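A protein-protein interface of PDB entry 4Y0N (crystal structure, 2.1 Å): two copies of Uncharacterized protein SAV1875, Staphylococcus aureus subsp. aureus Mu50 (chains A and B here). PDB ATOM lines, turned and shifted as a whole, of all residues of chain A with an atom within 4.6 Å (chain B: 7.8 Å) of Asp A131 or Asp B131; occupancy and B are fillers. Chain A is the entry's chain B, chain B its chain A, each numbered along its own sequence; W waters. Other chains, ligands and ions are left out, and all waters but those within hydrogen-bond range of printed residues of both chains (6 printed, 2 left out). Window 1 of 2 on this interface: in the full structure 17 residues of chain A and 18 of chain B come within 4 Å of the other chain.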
ATOM      1  N   ARG A  80     -20.424  16.522  22.497  1.00  0.00           N
ATOM      2  CA  ARG A  80     -21.450  15.539  22.182  1.00  0.00           C
ATOM      3  C   ARG A  80     -22.520  15.460  23.248  1.00  0.00           C
ATOM      4  O   ARG A  80     -23.541  14.807  23.053  1.00  0.00           O
ATOM      5  CB  ARG A  80     -20.839  14.154  21.926  1.00  0.00           C
ATOM      6  CG  ARG A  80     -19.945  14.124  20.696  1.00  0.00           C
ATOM      7  CD  ARG A  80     -19.304  12.753  20.511  1.00  0.00           C
ATOM      8  NE  ARG A  80     -20.128  11.866  19.687  1.00  0.00           N
ATOM      9  CZ  ARG A  80     -20.039  10.535  19.695  1.00  0.00           C
ATOM     10  NH1 ARG A  80     -19.206   9.916  20.536  1.00  0.00           N
ATOM     11  NH2 ARG A  80     -20.750   9.823  18.829  1.00  0.00           N
ATOM     12  N   ILE A 112     -18.701  11.184  13.927  1.00  0.00           N
ATOM     13  CA  ILE A 112     -19.668  10.086  14.053  1.00  0.00           C
ATOM     14  C   ILE A 112     -21.109  10.609  14.030  1.00  0.00           C
ATOM     15  O   ILE A 112     -21.994  10.031  13.367  1.00  0.00           O
ATOM     16  CB  ILE A 112     -19.438   9.261  15.345  1.00  0.00           C
ATOM     17  CG1 ILE A 112     -18.192   8.374  15.220  1.00  0.00           C
ATOM     18  CG2 ILE A 112     -20.641   8.383  15.634  1.00  0.00           C
ATOM     19  CD1 ILE A 112     -17.677   7.879  16.568  1.00  0.00           C
ATOM     20  N   ASN A 127      -8.816   4.629  21.706  1.00  0.00           N
ATOM     21  CA  ASN A 127     -10.017   4.598  22.553  1.00  0.00           C
ATOM     22  C   ASN A 127     -11.335   4.722  21.767  1.00  0.00           C
ATOM     23  O   ASN A 127     -12.402   4.333  22.258  1.00  0.00           O
ATOM     24  CB  ASN A 127      -9.965   5.698  23.631  1.00  0.00           C
ATOM     25  CG  ASN A 127      -8.618   5.779  24.346  1.00  0.00           C
ATOM     26  OD1 ASN A 127      -8.564   5.897  25.573  1.00  0.00           O
ATOM     27  ND2 ASN A 127      -7.553   5.876  23.584  1.00  0.00           N
ATOM     28  N   VAL A 128     -11.267   5.296  20.568  1.00  0.00           N
ATOM     29  CA  VAL A 128     -12.493   5.616  19.815  1.00  0.00           C
ATOM     30  C   VAL A 128     -12.601   4.860  18.489  1.00  0.00           C
ATOM     31  O   VAL A 128     -13.597   4.993  17.761  1.00  0.00           O
ATOM     32  CB  VAL A 128     -12.662   7.136  19.580  1.00  0.00           C
ATOM     33  CG1 VAL A 128     -12.460   7.915  20.873  1.00  0.00           C
ATOM     34  CG2 VAL A 128     -11.693   7.631  18.524  1.00  0.00           C
ATOM     35  N   ARG A 129     -11.608   4.020  18.207  1.00  0.00           N
ATOM     36  CA  ARG A 129     -11.539   3.307  16.928  1.00  0.00           C
ATOM     37  C   ARG A 129     -12.711   2.359  16.701  1.00  0.00           C
ATOM     38  O   ARG A 129     -13.288   2.319  15.613  1.00  0.00           O
ATOM     39  CB  ARG A 129     -10.215   2.544  16.807  1.00  0.00           C
ATOM     40  CG  ARG A 129      -9.077   3.464  16.400  1.00  0.00           C
ATOM     41  CD  ARG A 129      -7.745   2.748  16.239  1.00  0.00           C
ATOM     42  NE  ARG A 129      -6.669   3.724  16.382  1.00  0.00           N
ATOM     43  CZ  ARG A 129      -5.411   3.423  16.697  1.00  0.00           C
ATOM     44  NH1 ARG A 129      -5.011   2.163  16.688  1.00  0.00           N
ATOM     45  NH2 ARG A 129      -4.519   4.398  16.857  1.00  0.00           N
ATOM     46  N   LYS A 130     -13.071   1.622  17.741  1.00  0.00           N
ATOM     47  CA  LYS A 130     -14.215   0.713  17.687  1.00  0.00           C
ATOM     48  C   LYS A 130     -15.498   1.467  17.307  1.00  0.00           C
ATOM     49  O   LYS A 130     -16.230   1.059  16.392  1.00  0.00           O
ATOM     50  CB  LYS A 130     -14.387   0.024  19.051  1.00  0.00           C
ATOM     51  CG  LYS A 130     -15.601  -0.880  19.133  1.00  0.00           C
ATOM     52  CD  LYS A 130     -15.562  -1.876  17.996  1.00  0.00           C
ATOM     53  CE  LYS A 130     -15.050  -3.212  18.493  1.00  0.00           C
ATOM     54  NZ  LYS A 130     -16.159  -4.199  18.465  1.00  0.00           N
ATOM     55  N   ASP A 131     -15.727   2.611  17.945  1.00  0.00           N
ATOM     56  CA  ASP A 131     -16.920   3.408  17.667  1.00  0.00           C
ATOM     57  C   ASP A 131     -16.920   3.970  16.221  1.00  0.00           C
ATOM     58  O   ASP A 131     -17.960   4.008  15.567  1.00  0.00           O
ATOM     59  CB  ASP A 131     -17.071   4.531  18.700  1.00  0.00           C
ATOM     60  CG  ASP A 131     -17.186   3.998  20.149  1.00  0.00           C
ATOM     61  OD1 ASP A 131     -17.591   2.820  20.343  1.00  0.00           O
ATOM     62  OD2 ASP A 131     -16.721   4.705  21.083  1.00  0.00           O
ATOM     63  N   LEU A 132     -15.748   4.341  15.706  1.00  0.00           N
ATOM     64  CA  LEU A 132     -15.652   4.774  14.308  1.00  0.00           C
ATOM     65  C   LEU A 132     -15.973   3.636  13.341  1.00  0.00           C
ATOM     66  O   LEU A 132     -16.613   3.862  12.303  1.00  0.00           O
ATOM     67  CB  LEU A 132     -14.266   5.361  13.987  1.00  0.00           C
ATOM     68  CG  LEU A 132     -13.969   6.716  14.633  1.00  0.00           C
ATOM     69  CD1 LEU A 132     -12.461   6.971  14.665  1.00  0.00           C
ATOM     70  CD2 LEU A 132     -14.718   7.840  13.904  1.00  0.00           C
ATOM     71  N   SER A 133     -15.471   2.436  13.645  1.00  0.00           N
ATOM     72  CA  SER A 133     -15.774   1.261  12.838  1.00  0.00           C
ATOM     73  C   SER A 133     -17.265   0.998  12.795  1.00  0.00           C
ATOM     74  O   SER A 133     -17.801   0.631  11.748  1.00  0.00           O
ATOM     75  CB  SER A 133     -15.071   0.020  13.390  1.00  0.00           C
ATOM     76  OG  SER A 133     -13.695   0.123  13.143  1.00  0.00           O
ATOM     77  N   ASN A 134     -17.869   0.952  13.974  1.00  0.00           N
ATOM     78  CA  ASN A 134     -19.307   0.769  14.101  1.00  0.00           C
ATOM     79  C   ASN A 134     -20.109   1.823  13.330  1.00  0.00           C
ATOM     80  O   ASN A 134     -21.220   1.549  12.890  1.00  0.00           O
ATOM     81  CB  ASN A 134     -19.703   0.768  15.587  1.00  0.00           C
ATOM     82  CG  ASN A 134     -19.469  -0.581  16.249  1.00  0.00           C
ATOM     83  OD1 ASN A 134     -19.174  -1.569  15.570  1.00  0.00           O
ATOM     84  ND2 ASN A 134     -19.563  -0.623  17.575  1.00  0.00           N
ATOM     85  N   ALA A 135     -19.534   3.011  13.140  1.00  0.00           N
ATOM     86  CA  ALA A 135     -20.177   4.057  12.325  1.00  0.00           C
ATOM     87  C   ALA A 135     -19.949   3.832  10.823  1.00  0.00           C
ATOM     88  O   ALA A 135     -20.378   4.638   9.988  1.00  0.00           O
ATOM     89  CB  ALA A 135     -19.681   5.448  12.735  1.00  0.00           C
ATOM     90  N   ASP B  77     -13.711   5.517  29.111  1.00  0.00           N
ATOM     91  CA  ASP B  77     -12.857   5.920  27.994  1.00  0.00           C
ATOM     92  C   ASP B  77     -11.381   5.570  28.257  1.00  0.00           C
ATOM     93  O   ASP B  77     -10.746   4.903  27.441  1.00  0.00           O
ATOM     94  CB  ASP B  77     -13.039   7.415  27.686  1.00  0.00           C
ATOM     95  CG  ASP B  77     -12.373   7.831  26.372  1.00  0.00           C
ATOM     96  OD1 ASP B  77     -13.104   8.164  25.413  1.00  0.00           O
ATOM     97  OD2 ASP B  77     -11.138   7.989  26.352  1.00  0.00           O
ATOM     98  N   ARG B  80     -10.912   1.861  27.793  1.00  0.00           N
ATOM     99  CA  ARG B  80     -10.891   1.487  26.376  1.00  0.00           C
ATOM    100  C   ARG B  80      -9.584   1.881  25.714  1.00  0.00           C
ATOM    101  O   ARG B  80      -9.357   1.577  24.551  1.00  0.00           O
ATOM    102  CB  ARG B  80     -12.095   2.091  25.632  1.00  0.00           C
ATOM    103  CG  ARG B  80     -13.444   1.639  26.189  1.00  0.00           C
ATOM    104  CD  ARG B  80     -14.605   2.327  25.483  1.00  0.00           C
ATOM    105  NE  ARG B  80     -14.959   1.658  24.232  1.00  0.00           N
ATOM    106  CZ  ARG B  80     -15.690   2.209  23.257  1.00  0.00           C
ATOM    107  NH1 ARG B  80     -16.047   3.492  23.319  1.00  0.00           N
ATOM    108  NH2 ARG B  80     -16.057   1.473  22.208  1.00  0.00           N
ATOM    109  N   PRO B 108     -21.661   2.310  29.741  1.00  0.00           N
ATOM    110  CA  PRO B 108     -22.003   1.357  28.689  1.00  0.00           C
ATOM    111  C   PRO B 108     -21.062   1.391  27.482  1.00  0.00           C
ATOM    112  O   PRO B 108     -21.082   0.458  26.671  1.00  0.00           O
ATOM    113  CB  PRO B 108     -23.431   1.779  28.289  1.00  0.00           C
ATOM    114  CG  PRO B 108     -23.991   2.372  29.543  1.00  0.00           C
ATOM    115  CD  PRO B 108     -22.831   3.100  30.171  1.00  0.00           C
ATOM    116  N   GLN B 109     -20.173   2.387  27.413  1.00  0.00           N
ATOM    117  CA  GLN B 109     -19.091   2.355  26.422  1.00  0.00           C
ATOM    118  C   GLN B 109     -18.310   1.034  26.457  1.00  0.00           C
ATOM    119  O   GLN B 109     -17.893   0.509  25.410  1.00  0.00           O
ATOM    120  CB  GLN B 109     -18.128   3.534  26.615  1.00  0.00           C
ATOM    121  CG  GLN B 109     -18.673   4.881  26.156  1.00  0.00           C
ATOM    122  CD  GLN B 109     -17.662   5.997  26.345  1.00  0.00           C
ATOM    123  OE1 GLN B 109     -17.186   6.244  27.458  1.00  0.00           O
ATOM    124  NE2 GLN B 109     -17.241   6.595  25.241  1.00  0.00           N
ATOM    125  N   ILE B 110     -18.041   0.526  27.651  1.00  0.00           N
ATOM    126  CA  ILE B 110     -17.280  -0.714  27.752  1.00  0.00           C
ATOM    127  C   ILE B 110     -18.058  -1.907  27.181  1.00  0.00           C
ATOM    128  O   ILE B 110     -17.480  -2.758  26.523  1.00  0.00           O
ATOM    129  CB  ILE B 110     -16.819  -0.990  29.199  1.00  0.00           C
ATOM    130  CG1 ILE B 110     -15.576  -0.165  29.511  1.00  0.00           C
ATOM    131  CG2 ILE B 110     -16.502  -2.468  29.395  1.00  0.00           C
ATOM    132  CD1 ILE B 110     -14.332  -0.707  28.832  1.00  0.00           C
ATOM    133  N   ILE B 112     -19.879  -1.834  24.621  1.00  0.00           N
ATOM    134  CA  ILE B 112     -19.753  -1.800  23.158  1.00  0.00           C
ATOM    135  C   ILE B 112     -18.656  -2.775  22.727  1.00  0.00           C
ATOM    136  O   ILE B 112     -18.786  -3.479  21.725  1.00  0.00           O
ATOM    137  CB  ILE B 112     -19.418  -0.376  22.637  1.00  0.00           C
ATOM    138  CG1 ILE B 112     -20.603   0.572  22.866  1.00  0.00           C
ATOM    139  CG2 ILE B 112     -19.025  -0.409  21.158  1.00  0.00           C
ATOM    140  CD1 ILE B 112     -20.251   2.038  22.655  1.00  0.00           C
ATOM    141  N   ASP B 113     -17.632  -2.903  23.565  1.00  0.00           N
ATOM    142  CA  ASP B 113     -16.449  -3.655  23.186  1.00  0.00           C
ATOM    143  C   ASP B 113     -16.667  -5.160  23.360  1.00  0.00           C
ATOM    144  O   ASP B 113     -15.809  -5.942  22.984  1.00  0.00           O
ATOM    145  CB  ASP B 113     -15.242  -3.194  24.010  1.00  0.00           C
ATOM    146  CG  ASP B 113     -14.743  -1.821  23.591  1.00  0.00           C
ATOM    147  OD1 ASP B 113     -15.078  -1.388  22.467  1.00  0.00           O
ATOM    148  OD2 ASP B 113     -14.016  -1.177  24.378  1.00  0.00           O
ATOM    149  N   LEU B 117     -24.123  -6.413  21.897  1.00  0.00           N
ATOM    150  CA  LEU B 117     -25.233  -5.504  22.162  1.00  0.00           C
ATOM    151  C   LEU B 117     -26.360  -5.572  21.125  1.00  0.00           C
ATOM    152  O   LEU B 117     -27.435  -5.008  21.344  1.00  0.00           O
ATOM    153  CB  LEU B 117     -24.741  -4.071  22.321  1.00  0.00           C
ATOM    154  CG  LEU B 117     -23.850  -3.795  23.525  1.00  0.00           C
ATOM    155  CD1 LEU B 117     -23.495  -2.307  23.620  1.00  0.00           C
ATOM    156  CD2 LEU B 117     -24.489  -4.300  24.815  1.00  0.00           C
ATOM    157  N   LEU B 126     -26.396  11.020  27.227  1.00  0.00           N
ATOM    158  CA  LEU B 126     -26.594  11.465  25.849  1.00  0.00           C
ATOM    159  C   LEU B 126     -25.312  11.309  25.011  1.00  0.00           C
ATOM    160  O   LEU B 126     -25.385  10.906  23.853  1.00  0.00           O
ATOM    161  CB  LEU B 126     -27.099  12.920  25.816  1.00  0.00           C
ATOM    162  CG  LEU B 126     -27.298  13.595  24.443  1.00  0.00           C
ATOM    163  CD1 LEU B 126     -28.455  12.985  23.650  1.00  0.00           C
ATOM    164  CD2 LEU B 126     -27.511  15.105  24.576  1.00  0.00           C
ATOM    165  N   ASN B 127     -24.144  11.579  25.610  1.00  0.00           N
ATOM    166  CA  ASN B 127     -22.884  11.712  24.844  1.00  0.00           C
ATOM    167  C   ASN B 127     -22.542  10.444  24.070  1.00  0.00           C
ATOM    168  O   ASN B 127     -21.634  10.441  23.239  1.00  0.00           O
ATOM    169  CB  ASN B 127     -21.695  12.007  25.771  1.00  0.00           C
ATOM    170  CG  ASN B 127     -21.932  13.198  26.672  1.00  0.00           C
ATOM    171  OD1 ASN B 127     -21.055  14.045  26.821  1.00  0.00           O
ATOM    172  ND2 ASN B 127     -23.112  13.264  27.294  1.00  0.00           N
ATOM    173  N   VAL B 128     -23.149   9.337  24.483  1.00  0.00           N
ATOM    174  CA  VAL B 128     -22.644   8.003  24.188  1.00  0.00           C
ATOM    175  C   VAL B 128     -23.733   7.208  23.450  1.00  0.00           C
ATOM    176  O   VAL B 128     -23.483   6.128  22.930  1.00  0.00           O
ATOM    177  CB  VAL B 128     -22.248   7.326  25.521  1.00  0.00           C
ATOM    178  CG1 VAL B 128     -22.776   5.913  25.644  1.00  0.00           C
ATOM    179  CG2 VAL B 128     -20.751   7.436  25.755  1.00  0.00           C
ATOM    180  N   ARG B 129     -24.919   7.800  23.333  1.00  0.00           N
ATOM    181  CA  ARG B 129     -26.092   7.098  22.821  1.00  0.00           C
ATOM    182  C   ARG B 129     -26.007   6.710  21.355  1.00  0.00           C
ATOM    183  O   ARG B 129     -26.419   5.615  20.964  1.00  0.00           O
ATOM    184  CB  ARG B 129     -27.346   7.932  23.049  1.00  0.00           C
ATOM    185  CG  ARG B 129     -27.959   7.678  24.408  1.00  0.00           C
ATOM    186  CD  ARG B 129     -29.194   8.536  24.603  1.00  0.00           C
ATOM    187  NE  ARG B 129     -29.316   8.807  26.016  1.00  0.00           N
ATOM    188  CZ  ARG B 129     -29.931   9.854  26.540  1.00  0.00           C
ATOM    189  NH1 ARG B 129     -30.619  10.703  25.771  1.00  0.00           N
ATOM    190  NH2 ARG B 129     -29.868  10.028  27.849  1.00  0.00           N
ATOM    191  N   LYS B 130     -25.503   7.624  20.541  1.00  0.00           N
ATOM    192  CA  LYS B 130     -25.239   7.323  19.156  1.00  0.00           C
ATOM    193  C   LYS B 130     -24.260   6.144  18.995  1.00  0.00           C
ATOM    194  O   LYS B 130     -24.505   5.239  18.200  1.00  0.00           O
ATOM    195  CB  LYS B 130     -24.732   8.566  18.425  1.00  0.00           C
ATOM    196  CG  LYS B 130     -24.271   8.294  17.005  1.00  0.00           C
ATOM    197  CD  LYS B 130     -25.453   8.025  16.093  1.00  0.00           C
ATOM    198  CE  LYS B 130     -26.085   9.348  15.678  1.00  0.00           C
ATOM    199  NZ  LYS B 130     -26.755   9.207  14.362  1.00  0.00           N
ATOM    200  N   ASP B 131     -23.157   6.160  19.731  1.00  0.00           N
ATOM    201  CA  ASP B 131     -22.203   5.048  19.668  1.00  0.00           C
ATOM    202  C   ASP B 131     -22.830   3.699  20.093  1.00  0.00           C
ATOM    203  O   ASP B 131     -22.568   2.662  19.490  1.00  0.00           O
ATOM    204  CB  ASP B 131     -20.933   5.368  20.481  1.00  0.00           C
ATOM    205  CG  ASP B 131     -20.147   6.565  19.902  1.00  0.00           C
ATOM    206  OD1 ASP B 131     -20.330   6.877  18.707  1.00  0.00           O
ATOM    207  OD2 ASP B 131     -19.448   7.275  20.668  1.00  0.00           O
ATOM    208  N   LEU B 132     -23.675   3.724  21.114  1.00  0.00           N
ATOM    209  CA  LEU B 132     -24.421   2.536  21.530  1.00  0.00           C
ATOM    210  C   LEU B 132     -25.336   2.047  20.400  1.00  0.00           C
ATOM    211  O   LEU B 132     -25.389   0.854  20.093  1.00  0.00           O
ATOM    212  CB  LEU B 132     -25.301   2.897  22.733  1.00  0.00           C
ATOM    213  CG  LEU B 132     -25.068   2.296  24.111  1.00  0.00           C
ATOM    214  CD1 LEU B 132     -23.619   1.875  24.311  1.00  0.00           C
ATOM    215  CD2 LEU B 132     -25.526   3.288  25.178  1.00  0.00           C
ATOM    216  N   SER B 133     -26.080   2.966  19.800  1.00  0.00           N
ATOM    217  CA  SER B 133     -26.888   2.624  18.629  1.00  0.00           C
ATOM    218  C   SER B 133     -26.086   2.042  17.455  1.00  0.00           C
ATOM    219  O   SER B 133     -26.551   1.116  16.782  1.00  0.00           O
ATOM    220  CB  SER B 133     -27.742   3.816  18.178  1.00  0.00           C
ATOM    221  OG  SER B 133     -28.812   3.362  17.356  1.00  0.00           O
ATOM    222  N   ASN B 134     -24.909   2.602  17.175  1.00  0.00           N
ATOM    223  CA  ASN B 134     -24.078   2.066  16.094  1.00  0.00           C
ATOM    224  C   ASN B 134     -23.529   0.679  16.444  1.00  0.00           C
ATOM    225  O   ASN B 134     -23.217  -0.115  15.559  1.00  0.00           O
ATOM    226  CB  ASN B 134     -22.938   3.028  15.728  1.00  0.00           C
ATOM    227  CG  ASN B 134     -23.428   4.254  14.967  1.00  0.00           C
ATOM    228  OD1 ASN B 134     -24.526   4.257  14.440  1.00  0.00           O
ATOM    229  ND2 ASN B 134     -22.623   5.307  14.937  1.00  0.00           N
ATOM    230  N   ALA B 135     -23.495   0.361  17.736  1.00  0.00           N
ATOM    231  CA  ALA B 135     -23.063  -0.957  18.187  1.00  0.00           C
ATOM    232  C   ALA B 135     -24.194  -1.978  18.102  1.00  0.00           C
ATOM    233  O   ALA B 135     -23.978  -3.155  18.374  1.00  0.00           O
ATOM    234  CB  ALA B 135     -22.529  -0.901  19.617  1.00  0.00           C
ATOM    235  N   GLY B 136     -25.397  -1.527  17.762  1.00  0.00           N
ATOM    236  CA  GLY B 136     -26.502  -2.439  17.486  1.00  0.00           C
ATOM    237  C   GLY B 136     -27.577  -2.473  18.560  1.00  0.00           C
ATOM    238  O   GLY B 136     -28.549  -3.209  18.433  1.00  0.00           O
ATOM    239  N   ALA B 137     -27.398  -1.684  19.625  1.00  0.00           N
ATOM    240  CA  ALA B 137     -28.366  -1.642  20.715  1.00  0.00           C
ATOM    241  C   ALA B 137     -29.652  -0.898  20.337  1.00  0.00           C
ATOM    242  O   ALA B 137     -29.614   0.071  19.580  1.00  0.00           O
ATOM    243  CB  ALA B 137     -27.734  -0.998  21.946  1.00  0.00           C
ATOM    244  N   VAL B 139     -31.524   1.777  21.797  1.00  0.00           N
ATOM    245  CA  VAL B 139     -31.181   2.767  22.820  1.00  0.00           C
ATOM    246  C   VAL B 139     -32.407   3.607  23.181  1.00  0.00           C
ATOM    247  O   VAL B 139     -33.122   4.088  22.306  1.00  0.00           O
ATOM    248  CB  VAL B 139     -30.045   3.711  22.369  1.00  0.00           C
ATOM    249  CG1 VAL B 139     -29.780   4.768  23.433  1.00  0.00           C
ATOM    250  CG2 VAL B 139     -28.769   2.923  22.082  1.00  0.00           C
HETATM  251  O   HOH W   1     -22.964   7.442  12.991  1.00  0.00           O
HETATM  252  O   HOH W   2     -18.758   5.829  22.868  1.00  0.00           O
HETATM  253  O   HOH W   3     -19.735  -3.197  19.137  1.00  0.00           O
HETATM  254  O   HOH W   4     -19.976   1.947  18.546  1.00  0.00           O
HETATM  255  O   HOH W   5     -14.070   5.391  24.396  1.00  0.00           O
HETATM  256  O   HOH W   6     -20.196   4.766  16.774  1.00  0.00           O
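NE of Arg B80 is in hydrogen-bond range of O of Gln B109 (3.4 Å). OD2 of Asp B113 lies within salt-bridge range of NE of Arg B80 (3.0 Å).
O of Asp B77 sits close to OD1 of Asn A127. The guanidinium group (NH1) of Arg B80 is in salt-bridge range of the side-chain carboxylate (OD2) of Asp A131 (2.6 Å). The side-chain carboxylate of Asp B131 lies within salt-bridge range of the guanidinium group of Arg A80 (2.7 Å).
Of the 21 printed residues of chain B, 9 touch a printed residue of chain A. Hydrophobic or aromatic side chains of chain B within 4 Å of the printed part of chain A: Ile B112 and Ala B135.
O of Arg A80 touches CA of Asn B127, at 3.6 Å. Lys B130 touches Ile A112 (CG to CG2, 3.9 Å). OD1 of Asp B131 touches CG2 of Ile A112, at 3.4 Å. Ile A112 touches Asn B134 (CG2 to ND2, 3.7 Å). Asn A127 touches Arg B80 (CA to O, 3.7 Å). OD1 of Asp B113 touches CG of Lys A130 (3.4 Å). Ile B112 touches Asp A131. Asn A134 touches Asn B134 (CB to O, 3.6 Å). Asn A134 touches Ala B135. Ala A135 touches Asn B134 (CB to ND2, 3.7 Å).
Arg A80 touches Asp B131, and with the chains exchanged Asp A131 touches Arg B80. Ile A112 touches Asn B134, and with the chains exchanged Asn A134 touches Ile B112. Asp A131 touches its own counterpart, Asp B131. Asn B134 touches its own counterpart, Asn A134. Of the 16 pairs that touch across the chains among the printed residues, 12 have their exchanged pair printed and touching as well.
Water W6 lies within hydrogen-bond range of O of Asp A131 (2.7 Å), OD1 of Asp B131 (2.9 Å) and ND2 of Asn B134 (3.1 Å). Water W2 lies within hydrogen-bond range of the side-chain carboxylate (OD2) of Asp B131 (2.7 Å), the side-chain amide nitrogen (NE2) of Gln B109 (2.9 Å) and the side-chain carboxylate (OD2) of Asp A131 (2.9 Å). Water W3 lies within hydrogen-bond range of the backbone carbonyl oxygen (O) of Ile B112 (2.8 Å) and the side-chain amide nitrogen (ND2) of Asn A134 (3.0 Å). Water W4 lies within hydrogen-bond range of the side-chain amide nitrogen (ND2) of Asn A134 (2.8 Å), the backbone carbonyl oxygen (O) of Asp B131 (2.8 Å) and the side-chain carboxylate (OD1) of Asp A131 (3.1 Å). Water W1 bridges O of Ile A112 (2.8 Å) and ND2 of Asn B134 (2.9 Å). Water W5 lies within hydrogen-bond range of O of Asn A127, NH1 of Arg B80, OD1 of Asp B77 and NE2 of Gln B109.
Asp A131 touches just these residues of chain B: Arg B80 (2.6 Å), Ile B112 (3.6 Å) and Asp B131 (3.8 Å). Printed residues of chain B within 4 Å of Ile A112: Lys B130 (3.9 Å), Asp B131 (3.4 Å) and Asn B134 (3.7 Å). Of the printed residues of chain A, Ala B135 touches Asn A134 (3.6 Å). Printed residues of chain B within 4 Å of Ala A135: Asn B134. Of the printed residues of chain A, Asp B77 touches Asn A127. The nearest residue of chain B that does not touch Asp A131 is Gln B109 (4.6 Å).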
